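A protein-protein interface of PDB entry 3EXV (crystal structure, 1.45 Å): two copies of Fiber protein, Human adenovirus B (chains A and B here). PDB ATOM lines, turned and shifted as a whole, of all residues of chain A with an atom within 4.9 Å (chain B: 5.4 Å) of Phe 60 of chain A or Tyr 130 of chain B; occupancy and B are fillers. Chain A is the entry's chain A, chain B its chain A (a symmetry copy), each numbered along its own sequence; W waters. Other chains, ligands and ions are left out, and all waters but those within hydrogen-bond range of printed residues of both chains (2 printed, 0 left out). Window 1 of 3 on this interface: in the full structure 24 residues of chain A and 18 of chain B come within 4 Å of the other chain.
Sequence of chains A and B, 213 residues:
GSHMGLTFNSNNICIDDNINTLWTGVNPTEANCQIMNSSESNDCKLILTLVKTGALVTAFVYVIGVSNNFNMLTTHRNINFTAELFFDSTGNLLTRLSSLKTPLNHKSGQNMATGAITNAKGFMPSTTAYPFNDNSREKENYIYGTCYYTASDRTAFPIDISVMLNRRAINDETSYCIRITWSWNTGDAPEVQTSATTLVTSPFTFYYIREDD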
ATOM      1  N   ILE A  47      -5.681  15.212 -13.583  1.00  0.00           N
ATOM      2  CA  ILE A  47      -6.114  14.127 -12.727  1.00  0.00           C
ATOM      3  C   ILE A  47      -7.308  14.632 -11.931  1.00  0.00           C
ATOM      4  O   ILE A  47      -7.187  15.573 -11.148  1.00  0.00           O
ATOM      5  CB  ILE A  47      -4.995  13.675 -11.766  1.00  0.00           C
ATOM      6  CG1 ILE A  47      -3.689  13.431 -12.533  1.00  0.00           C
ATOM      7  CG2 ILE A  47      -5.410  12.415 -11.016  1.00  0.00           C
ATOM      8  CD1 ILE A  47      -3.800  12.392 -13.641  1.00  0.00           C
ATOM      9  N   LEU A  48      -8.468  14.028 -12.169  1.00  0.00           N
ATOM     10  CA  LEU A  48      -9.708  14.453 -11.534  1.00  0.00           C
ATOM     11  C   LEU A  48     -10.444  13.243 -11.000  1.00  0.00           C
ATOM     12  O   LEU A  48     -10.706  12.297 -11.742  1.00  0.00           O
ATOM     13  CB  LEU A  48     -10.593  15.195 -12.540  1.00  0.00           C
ATOM     14  CG  LEU A  48     -11.957  15.673 -12.026  1.00  0.00           C
ATOM     15  CD1 LEU A  48     -11.789  16.712 -10.928  1.00  0.00           C
ATOM     16  CD2 LEU A  48     -12.793  16.229 -13.169  1.00  0.00           C
ATOM     17  N   THR A  49     -10.766  13.275  -9.710  1.00  0.00           N
ATOM     18  CA  THR A  49     -11.507  12.200  -9.065  1.00  0.00           C
ATOM     19  C   THR A  49     -12.726  12.779  -8.359  1.00  0.00           C
ATOM     20  O   THR A  49     -12.594  13.630  -7.480  1.00  0.00           O
ATOM     21  CB  THR A  49     -10.633  11.452  -8.036  1.00  0.00           C
ATOM     22  OG1 THR A  49      -9.445  10.968  -8.673  1.00  0.00           O
ATOM     23  CG2 THR A  49     -11.394  10.282  -7.428  1.00  0.00           C
ATOM     24  N   THR A  58     -17.168  14.771  -3.388  1.00  0.00           N
ATOM     25  CA  THR A  58     -15.809  15.122  -3.015  1.00  0.00           C
ATOM     26  C   THR A  58     -14.995  15.157  -4.294  1.00  0.00           C
ATOM     27  O   THR A  58     -14.864  14.140  -4.972  1.00  0.00           O
ATOM     28  CB  THR A  58     -15.210  14.089  -2.048  1.00  0.00           C
ATOM     29  OG1 THR A  58     -15.979  14.062  -0.841  1.00  0.00           O
ATOM     30  CG2 THR A  58     -13.762  14.431  -1.718  1.00  0.00           C
ATOM     31  N   ALA A  59     -14.474  16.336  -4.636  1.00  0.00           N
ATOM     32  CA  ALA A  59     -13.750  16.536  -5.892  1.00  0.00           C
ATOM     33  C   ALA A  59     -12.267  16.749  -5.618  1.00  0.00           C
ATOM     34  O   ALA A  59     -11.895  17.623  -4.850  1.00  0.00           O
ATOM     35  CB  ALA A  59     -14.325  17.718  -6.652  1.00  0.00           C
ATOM     36  N   PHE A  60     -11.438  15.963  -6.296  1.00  0.00           N
ATOM     37  CA  PHE A  60     -10.008  15.868  -6.024  1.00  0.00           C
ATOM     38  C   PHE A  60      -9.294  16.086  -7.354  1.00  0.00           C
ATOM     39  O   PHE A  60      -9.474  15.304  -8.281  1.00  0.00           O
ATOM     40  CB  PHE A  60      -9.748  14.470  -5.442  1.00  0.00           C
ATOM     41  CG  PHE A  60      -8.299  14.105  -5.271  1.00  0.00           C
ATOM     42  CD1 PHE A  60      -7.663  14.282  -4.047  1.00  0.00           C
ATOM     43  CD2 PHE A  60      -7.608  13.469  -6.293  1.00  0.00           C
ATOM     44  CE1 PHE A  60      -6.343  13.889  -3.869  1.00  0.00           C
ATOM     45  CE2 PHE A  60      -6.291  13.080  -6.124  1.00  0.00           C
ATOM     46  CZ  PHE A  60      -5.658  13.289  -4.909  1.00  0.00           C
ATOM     47  N   VAL A  61      -8.529  17.174  -7.470  1.00  0.00           N
ATOM     48  CA  VAL A  61      -8.008  17.591  -8.776  1.00  0.00           C
ATOM     49  C   VAL A  61      -6.584  18.157  -8.741  1.00  0.00           C
ATOM     50  O   VAL A  61      -6.212  18.889  -7.821  1.00  0.00           O
ATOM     51  CB  VAL A  61      -8.948  18.647  -9.424  1.00  0.00           C
ATOM     52  CG1 VAL A  61      -8.932  19.953  -8.625  1.00  0.00           C
ATOM     53  CG2 VAL A  61      -8.564  18.889 -10.875  1.00  0.00           C
ATOM     54  N   TYR A  62      -5.792  17.803  -9.753  1.00  0.00           N
ATOM     55  CA  TYR A  62      -4.491  18.436  -9.981  1.00  0.00           C
ATOM     56  C   TYR A  62      -4.024  18.224 -11.412  1.00  0.00           C
ATOM     57  O   TYR A  62      -4.643  17.480 -12.174  1.00  0.00           O
ATOM     58  CB  TYR A  62      -3.432  17.938  -8.988  1.00  0.00           C
ATOM     59  CG  TYR A  62      -3.122  16.455  -9.035  1.00  0.00           C
ATOM     60  CD1 TYR A  62      -3.991  15.524  -8.476  1.00  0.00           C
ATOM     61  CD2 TYR A  62      -1.928  15.988  -9.584  1.00  0.00           C
ATOM     62  CE1 TYR A  62      -3.698  14.166  -8.492  1.00  0.00           C
ATOM     63  CE2 TYR A  62      -1.625  14.627  -9.603  1.00  0.00           C
ATOM     64  CZ  TYR A  62      -2.515  13.723  -9.056  1.00  0.00           C
ATOM     65  OH  TYR A  62      -2.223  12.375  -9.064  1.00  0.00           O
ATOM     66  N   PRO A 203      -2.599  18.085  -5.048  1.00  0.00           N
ATOM     67  CA  PRO A 203      -4.037  17.835  -5.139  1.00  0.00           C
ATOM     68  C   PRO A 203      -4.873  18.850  -4.360  1.00  0.00           C
ATOM     69  O   PRO A 203      -4.579  19.140  -3.197  1.00  0.00           O
ATOM     70  CB  PRO A 203      -4.190  16.434  -4.535  1.00  0.00           C
ATOM     71  CG  PRO A 203      -2.858  15.812  -4.662  1.00  0.00           C
ATOM     72  CD  PRO A 203      -1.872  16.915  -4.525  1.00  0.00           C
ATOM     73  N   PHE A 204      -5.881  19.409  -5.024  1.00  0.00           N
ATOM     74  CA  PHE A 204      -6.849  20.269  -4.368  1.00  0.00           C
ATOM     75  C   PHE A 204      -8.155  19.516  -4.239  1.00  0.00           C
ATOM     76  O   PHE A 204      -8.659  18.962  -5.218  1.00  0.00           O
ATOM     77  CB  PHE A 204      -7.073  21.552  -5.163  1.00  0.00           C
ATOM     78  CG  PHE A 204      -8.107  22.465  -4.558  1.00  0.00           C
ATOM     79  CD1 PHE A 204      -7.920  22.998  -3.292  1.00  0.00           C
ATOM     80  CD2 PHE A 204      -9.265  22.793  -5.254  1.00  0.00           C
ATOM     81  CE1 PHE A 204      -8.869  23.833  -2.726  1.00  0.00           C
ATOM     82  CE2 PHE A 204     -10.215  23.634  -4.694  1.00  0.00           C
ATOM     83  CZ  PHE A 204     -10.016  24.154  -3.428  1.00  0.00           C
ATOM     84  N   THR A 205      -8.692  19.476  -3.024  1.00  0.00           N
ATOM     85  CA  THR A 205      -9.960  18.822  -2.776  1.00  0.00           C
ATOM     86  C   THR A 205     -11.014  19.858  -2.425  1.00  0.00           C
ATOM     87  O   THR A 205     -10.814  20.675  -1.525  1.00  0.00           O
ATOM     88  CB  THR A 205      -9.846  17.795  -1.644  1.00  0.00           C
ATOM     89  OG1 THR A 205      -8.889  16.796  -2.007  1.00  0.00           O
ATOM     90  CG2 THR A 205     -11.189  17.131  -1.383  1.00  0.00           C
ATOM     91  N   LEU B  56     -10.346   7.262  -3.158  1.00  0.00           N
ATOM     92  CA  LEU B  56      -9.470   8.024  -2.280  1.00  0.00           C
ATOM     93  C   LEU B  56      -9.503   7.514  -0.849  1.00  0.00           C
ATOM     94  O   LEU B  56     -10.428   6.805  -0.444  1.00  0.00           O
ATOM     95  CB  LEU B  56      -9.888   9.499  -2.271  1.00  0.00           C
ATOM     96  CG  LEU B  56     -10.045  10.199  -3.620  1.00  0.00           C
ATOM     97  CD1 LEU B  56     -10.623  11.593  -3.421  1.00  0.00           C
ATOM     98  CD2 LEU B  56      -8.717  10.265  -4.358  1.00  0.00           C
ATOM     99  N   PRO B 125      -1.191   4.552   0.452  1.00  0.00           N
ATOM    100  CA  PRO B 125      -1.007   5.449  -0.687  1.00  0.00           C
ATOM    101  C   PRO B 125      -0.581   4.685  -1.935  1.00  0.00           C
ATOM    102  O   PRO B 125       0.369   3.902  -1.889  1.00  0.00           O
ATOM    103  CB  PRO B 125       0.108   6.394  -0.221  1.00  0.00           C
ATOM    104  CG  PRO B 125       0.837   5.639   0.829  1.00  0.00           C
ATOM    105  CD  PRO B 125      -0.186   4.785   1.507  1.00  0.00           C
ATOM    106  N   SER B 126      -1.286   4.916  -3.037  1.00  0.00           N
ATOM    107  CA  SER B 126      -1.028   4.213  -4.293  1.00  0.00           C
ATOM    108  C   SER B 126       0.418   4.365  -4.755  1.00  0.00           C
ATOM    109  O   SER B 126       0.939   5.475  -4.826  1.00  0.00           O
ATOM    110  CB  SER B 126      -1.964   4.728  -5.389  1.00  0.00           C
ATOM    111  OG  SER B 126      -1.537   4.291  -6.665  1.00  0.00           O
ATOM    112  N   THR B 127       1.053   3.242  -5.088  1.00  0.00           N
ATOM    113  CA  THR B 127       2.406   3.258  -5.640  1.00  0.00           C
ATOM    114  C   THR B 127       2.394   3.634  -7.125  1.00  0.00           C
ATOM    115  O   THR B 127       3.444   3.890  -7.711  1.00  0.00           O
ATOM    116  CB  THR B 127       3.105   1.897  -5.466  1.00  0.00           C
ATOM    117  OG1 THR B 127       2.274   0.853  -5.988  1.00  0.00           O
ATOM    118  CG2 THR B 127       3.392   1.632  -3.996  1.00  0.00           C
ATOM    119  N   THR B 128       1.204   3.656  -7.725  1.00  0.00           N
ATOM    120  CA  THR B 128       1.038   4.116  -9.103  1.00  0.00           C
ATOM    121  C   THR B 128       0.924   5.642  -9.149  1.00  0.00           C
ATOM    122  O   THR B 128       1.499   6.281 -10.022  1.00  0.00           O
ATOM    123  CB  THR B 128      -0.204   3.484  -9.757  1.00  0.00           C
ATOM    124  OG1 THR B 128      -0.112   2.056  -9.671  1.00  0.00           O
ATOM    125  CG2 THR B 128      -0.316   3.898 -11.223  1.00  0.00           C
ATOM    126  N   ALA B 129       0.184   6.214  -8.200  1.00  0.00           N
ATOM    127  CA  ALA B 129       0.033   7.671  -8.103  1.00  0.00           C
ATOM    128  C   ALA B 129       1.225   8.326  -7.397  1.00  0.00           C
ATOM    129  O   ALA B 129       1.584   9.465  -7.703  1.00  0.00           O
ATOM    130  CB  ALA B 129      -1.256   8.018  -7.373  1.00  0.00           C
ATOM    131  N   TYR B 130       1.817   7.607  -6.442  1.00  0.00           N
ATOM    132  CA  TYR B 130       2.922   8.129  -5.636  1.00  0.00           C
ATOM    133  C   TYR B 130       4.097   7.150  -5.685  1.00  0.00           C
ATOM    134  O   TYR B 130       4.209   6.264  -4.844  1.00  0.00           O
ATOM    135  CB  TYR B 130       2.451   8.357  -4.195  1.00  0.00           C
ATOM    136  CG  TYR B 130       1.105   9.036  -4.141  1.00  0.00           C
ATOM    137  CD1 TYR B 130      -0.041   8.331  -3.788  1.00  0.00           C
ATOM    138  CD2 TYR B 130       0.964  10.364  -4.521  1.00  0.00           C
ATOM    139  CE1 TYR B 130      -1.281   8.942  -3.777  1.00  0.00           C
ATOM    140  CE2 TYR B 130      -0.272  10.983  -4.513  1.00  0.00           C
ATOM    141  CZ  TYR B 130      -1.392  10.268  -4.139  1.00  0.00           C
ATOM    142  OH  TYR B 130      -2.624  10.876  -4.133  1.00  0.00           O
ATOM    143  N   PRO B 131       4.973   7.303  -6.693  1.00  0.00           N
ATOM    144  CA  PRO B 131       6.036   6.326  -6.923  1.00  0.00           C
ATOM    145  C   PRO B 131       7.185   6.414  -5.923  1.00  0.00           C
ATOM    146  O   PRO B 131       7.240   7.340  -5.108  1.00  0.00           O
ATOM    147  CB  PRO B 131       6.530   6.681  -8.331  1.00  0.00           C
ATOM    148  CG  PRO B 131       6.254   8.128  -8.472  1.00  0.00           C
ATOM    149  CD  PRO B 131       5.009   8.403  -7.678  1.00  0.00           C
ATOM    150  N   PHE B 132       8.087   5.436  -5.991  1.00  0.00           N
ATOM    151  CA  PHE B 132       9.312   5.441  -5.205  1.00  0.00           C
ATOM    152  C   PHE B 132      10.515   5.797  -6.077  1.00  0.00           C
ATOM    153  O   PHE B 132      10.640   5.308  -7.197  1.00  0.00           O
ATOM    154  CB  PHE B 132       9.553   4.062  -4.575  1.00  0.00           C
ATOM    155  CG  PHE B 132       8.780   3.826  -3.312  1.00  0.00           C
ATOM    156  CD1 PHE B 132       7.580   3.129  -3.334  1.00  0.00           C
ATOM    157  CD2 PHE B 132       9.259   4.287  -2.094  1.00  0.00           C
ATOM    158  CE1 PHE B 132       6.869   2.902  -2.166  1.00  0.00           C
ATOM    159  CE2 PHE B 132       8.550   4.064  -0.920  1.00  0.00           C
ATOM    160  CZ  PHE B 132       7.355   3.372  -0.957  1.00  0.00           C
ATOM    161  N   ARG B 137       9.128  12.367 -11.379  1.00  0.00           N
ATOM    162  CA  ARG B 137       7.747  12.450 -10.896  1.00  0.00           C
ATOM    163  C   ARG B 137       7.658  12.889  -9.429  1.00  0.00           C
ATOM    164  O   ARG B 137       6.585  12.829  -8.831  1.00  0.00           O
ATOM    165  CB  ARG B 137       7.057  11.093 -11.044  1.00  0.00           C
ATOM    166  CG  ARG B 137       6.802  10.655 -12.475  1.00  0.00           C
ATOM    167  CD  ARG B 137       6.023   9.347 -12.506  1.00  0.00           C
ATOM    168  NE  ARG B 137       4.712   9.491 -11.871  1.00  0.00           N
ATOM    169  CZ  ARG B 137       3.941   8.482 -11.470  1.00  0.00           C
ATOM    170  NH1 ARG B 137       4.330   7.219 -11.623  1.00  0.00           N
ATOM    171  NH2 ARG B 137       2.769   8.743 -10.903  1.00  0.00           N
ATOM    172  N   GLU B 140       4.824  14.893  -7.606  1.00  0.00           N
ATOM    173  CA  GLU B 140       3.537  14.223  -7.402  1.00  0.00           C
ATOM    174  C   GLU B 140       3.420  13.553  -6.027  1.00  0.00           C
ATOM    175  O   GLU B 140       2.322  13.204  -5.599  1.00  0.00           O
ATOM    176  CB  GLU B 140       3.309  13.179  -8.498  1.00  0.00           C
ATOM    177  CG  GLU B 140       3.256  13.760  -9.901  1.00  0.00           C
ATOM    178  CD  GLU B 140       3.209  12.693 -10.971  1.00  0.00           C
ATOM    179  OE1 GLU B 140       2.382  11.767 -10.851  1.00  0.00           O
ATOM    180  OE2 GLU B 140       3.993  12.785 -11.940  1.00  0.00           O
ATOM    181  N   ASN B 141       4.549  13.379  -5.342  1.00  0.00           N
ATOM    182  CA  ASN B 141       4.569  12.704  -4.041  1.00  0.00           C
ATOM    183  C   ASN B 141       4.175  13.607  -2.869  1.00  0.00           C
ATOM    184  O   ASN B 141       4.108  13.143  -1.732  1.00  0.00           O
ATOM    185  CB  ASN B 141       5.963  12.125  -3.773  1.00  0.00           C
ATOM    186  CG  ASN B 141       6.324  11.005  -4.724  1.00  0.00           C
ATOM    187  OD1 ASN B 141       7.022  11.219  -5.715  1.00  0.00           O
ATOM    188  ND2 ASN B 141       5.845   9.802  -4.432  1.00  0.00           N
ATOM    189  N   ILE B 143       1.834  16.523  -0.711  1.00  0.00           N
ATOM    190  CA  ILE B 143       0.602  17.225  -0.370  1.00  0.00           C
ATOM    191  C   ILE B 143       0.945  18.280   0.681  1.00  0.00           C
ATOM    192  O   ILE B 143       1.800  18.047   1.537  1.00  0.00           O
ATOM    193  CB  ILE B 143      -0.459  16.265   0.205  1.00  0.00           C
ATOM    194  CG1 ILE B 143      -0.866  15.226  -0.840  1.00  0.00           C
ATOM    195  CG2 ILE B 143      -1.684  17.041   0.676  1.00  0.00           C
ATOM    196  CD1 ILE B 143      -1.657  14.072  -0.269  1.00  0.00           C
ATOM    197  N   LEU B 165       4.223  11.150   0.326  1.00  0.00           N
ATOM    198  CA  LEU B 165       3.749   9.776   0.215  1.00  0.00           C
ATOM    199  C   LEU B 165       4.757   8.943  -0.561  1.00  0.00           C
ATOM    200  O   LEU B 165       5.249   9.374  -1.600  1.00  0.00           O
ATOM    201  CB  LEU B 165       2.392   9.742  -0.485  1.00  0.00           C
ATOM    202  CG  LEU B 165       1.287  10.541   0.209  1.00  0.00           C
ATOM    203  CD1 LEU B 165       0.033  10.568  -0.646  1.00  0.00           C
ATOM    204  CD2 LEU B 165       0.990   9.963   1.587  1.00  0.00           C
ATOM    205  N   ASN B 166       5.067   7.756  -0.040  1.00  0.00           N
ATOM    206  CA  ASN B 166       6.040   6.857  -0.664  1.00  0.00           C
ATOM    207  C   ASN B 166       7.367   7.595  -0.946  1.00  0.00           C
ATOM    208  O   ASN B 166       7.997   8.085  -0.007  1.00  0.00           O
ATOM    209  CB  ASN B 166       5.433   6.204  -1.919  1.00  0.00           C
ATOM    210  CG  ASN B 166       4.184   5.367  -1.600  1.00  0.00           C
ATOM    211  OD1 ASN B 166       3.310   5.174  -2.449  1.00  0.00           O
ATOM    212  ND2 ASN B 166       4.104   4.876  -0.376  1.00  0.00           N
ATOM    213  N   ARG B 167       7.789   7.661  -2.214  1.00  0.00           N
ATOM    214  CA  ARG B 167       8.978   8.446  -2.628  1.00  0.00           C
ATOM    215  C   ARG B 167      10.320   7.844  -2.195  1.00  0.00           C
ATOM    216  O   ARG B 167      11.187   7.590  -3.032  1.00  0.00           O
ATOM    217  CB  ARG B 167       8.880   9.898  -2.130  1.00  0.00           C
ATOM    218  CG  ARG B 167      10.046  10.794  -2.550  1.00  0.00           C
ATOM    219  CD  ARG B 167      10.013  11.115  -4.024  1.00  0.00           C
ATOM    220  NE  ARG B 167      11.166  11.929  -4.421  1.00  0.00           N
ATOM    221  CZ  ARG B 167      12.235  11.481  -5.082  1.00  0.00           C
ATOM    222  NH1 ARG B 167      12.328  10.212  -5.462  1.00  0.00           N
ATOM    223  NH2 ARG B 167      13.219  12.320  -5.381  1.00  0.00           N
ATOM    224  N   TYR B 207      -6.111  14.168   1.357  1.00  0.00           N
ATOM    225  CA  TYR B 207      -6.649  13.100   0.534  1.00  0.00           C
ATOM    226  C   TYR B 207      -5.574  12.545  -0.368  1.00  0.00           C
ATOM    227  O   TYR B 207      -4.690  13.275  -0.819  1.00  0.00           O
ATOM    228  CB  TYR B 207      -7.802  13.625  -0.323  1.00  0.00           C
ATOM    229  CG  TYR B 207      -8.905  14.260   0.477  1.00  0.00           C
ATOM    230  CD1 TYR B 207     -10.060  13.555   0.786  1.00  0.00           C
ATOM    231  CD2 TYR B 207      -8.786  15.567   0.941  1.00  0.00           C
ATOM    232  CE1 TYR B 207     -11.075  14.137   1.531  1.00  0.00           C
ATOM    233  CE2 TYR B 207      -9.789  16.154   1.690  1.00  0.00           C
ATOM    234  CZ  TYR B 207     -10.933  15.435   1.979  1.00  0.00           C
ATOM    235  OH  TYR B 207     -11.931  16.022   2.720  1.00  0.00           O
ATOM    236  N   TYR B 208      -5.642  11.247  -0.626  1.00  0.00           N
ATOM    237  CA  TYR B 208      -4.757  10.631  -1.598  1.00  0.00           C
ATOM    238  C   TYR B 208      -5.421   9.460  -2.292  1.00  0.00           C
ATOM    239  O   TYR B 208      -6.373   8.870  -1.773  1.00  0.00           O
ATOM    240  CB  TYR B 208      -3.423  10.203  -0.957  1.00  0.00           C
ATOM    241  CG  TYR B 208      -3.516   9.242   0.219  1.00  0.00           C
ATOM    242  CD1 TYR B 208      -3.633   7.868   0.020  1.00  0.00           C
ATOM    243  CD2 TYR B 208      -3.419   9.706   1.528  1.00  0.00           C
ATOM    244  CE1 TYR B 208      -3.685   6.985   1.095  1.00  0.00           C
ATOM    245  CE2 TYR B 208      -3.471   8.834   2.607  1.00  0.00           C
ATOM    246  CZ  TYR B 208      -3.603   7.476   2.386  1.00  0.00           C
ATOM    247  OH  TYR B 208      -3.648   6.608   3.459  1.00  0.00           O
ATOM    248  N   ILE B 209      -4.933   9.159  -3.491  1.00  0.00           N
ATOM    249  CA  ILE B 209      -5.403   8.022  -4.262  1.00  0.00           C
ATOM    250  C   ILE B 209      -4.890   6.756  -3.596  1.00  0.00           C
ATOM    251  O   ILE B 209      -3.691   6.622  -3.344  1.00  0.00           O
ATOM    252  CB  ILE B 209      -4.910   8.096  -5.718  1.00  0.00           C
ATOM    253  CG1 ILE B 209      -5.552   9.291  -6.428  1.00  0.00           C
ATOM    254  CG2 ILE B 209      -5.229   6.806  -6.459  1.00  0.00           C
ATOM    255  CD1 ILE B 209      -4.907   9.638  -7.745  1.00  0.00           C
HETATM  256  O   HOH W   1      -2.497  12.542  -6.135  1.00  0.00           O
HETATM  257  O   HOH W   2       0.214  11.216  -9.331  1.00  0.00           O
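Among the printed residues, merely in contact across the chains: Phe 60 of chain A with Leu 56 of chain B, Phe 60 of chain A with Tyr 130 of chain B, Phe 60 of chain A with Tyr 207 of chain B, Phe 60 of chain A with Ile 209 of chain B and Thr 205 of chain A with Tyr 207 of chain B.
Phe 60 of chain A touches just these residues of chain B: Leu 56 (3.6 Å), Tyr 130 (3.95 Å), Tyr 207 (3.5 Å) and Ile 209 (3.9 Å). Val 61 of chain A touches none of the printed residues of chain B. Printed residues of chain B within 4 Å of Thr 205 of chain A: Tyr 207. Of the printed residues of chain A, Leu 56 of chain B touches Phe 60 (3.6 Å). Pro 131 of chain B touches none of the printed residues of chain A. Printed residues of chain A within 4 Å of Tyr 207 of chain B: Phe 60 and Thr 205. Of the printed residues of chain A, Ile 209 of chain B touches Phe 60 (3.9 Å). The nearest residue of chain B that does not touch Phe 60 of chain A is Tyr 208 of chain B (4.2 Å). The nearest printed residue of chain A that does not touch Tyr 130 of chain B is Pro 203 of chain A (5.0 Å).
Water W1 bridges the side-chain hydroxyl of Tyr 130 of chain B and the side-chain hydroxyl of Tyr 62 of chain A. Water W2 lies within hydrogen-bond range of OE1 of Glu 140 of chain B, OH of Tyr 62 of chain A and O of Ala 129 of chain B.
Of the 11 printed residues of chain A, 2 touch a printed residue of chain B. Hydrophobic or aromatic side chains of chain A that line the printed part of chain B: Phe 60. Among the printed residues, 5 pairs touch across the chains. Among the printed residues, no Asp or Glu carboxylate lies within 4 Å of a Lys or Arg side-chain nitrogen of the other chain.
The backbone NH (N) of Thr 49 of chain A lies within hydrogen-bond range of the backbone carbonyl oxygen (O) of Phe 60 of chain A. N of Ser 126 of chain B lies within hydrogen-bond range of O of Ile 209 of chain B (3.0 Å). O of Tyr 130 of chain B lies close to OD1 of Asn 166 of chain B, at 2.8 Å. N of Ile 209 of chain B is in hydrogen-bond range of OH of Tyr 130 of chain B (2.9 Å).
No position is printed for both chains. Of the 5 pairs that touch across the chains among the printed residues, none has its exchanged pair printed and touching as well.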
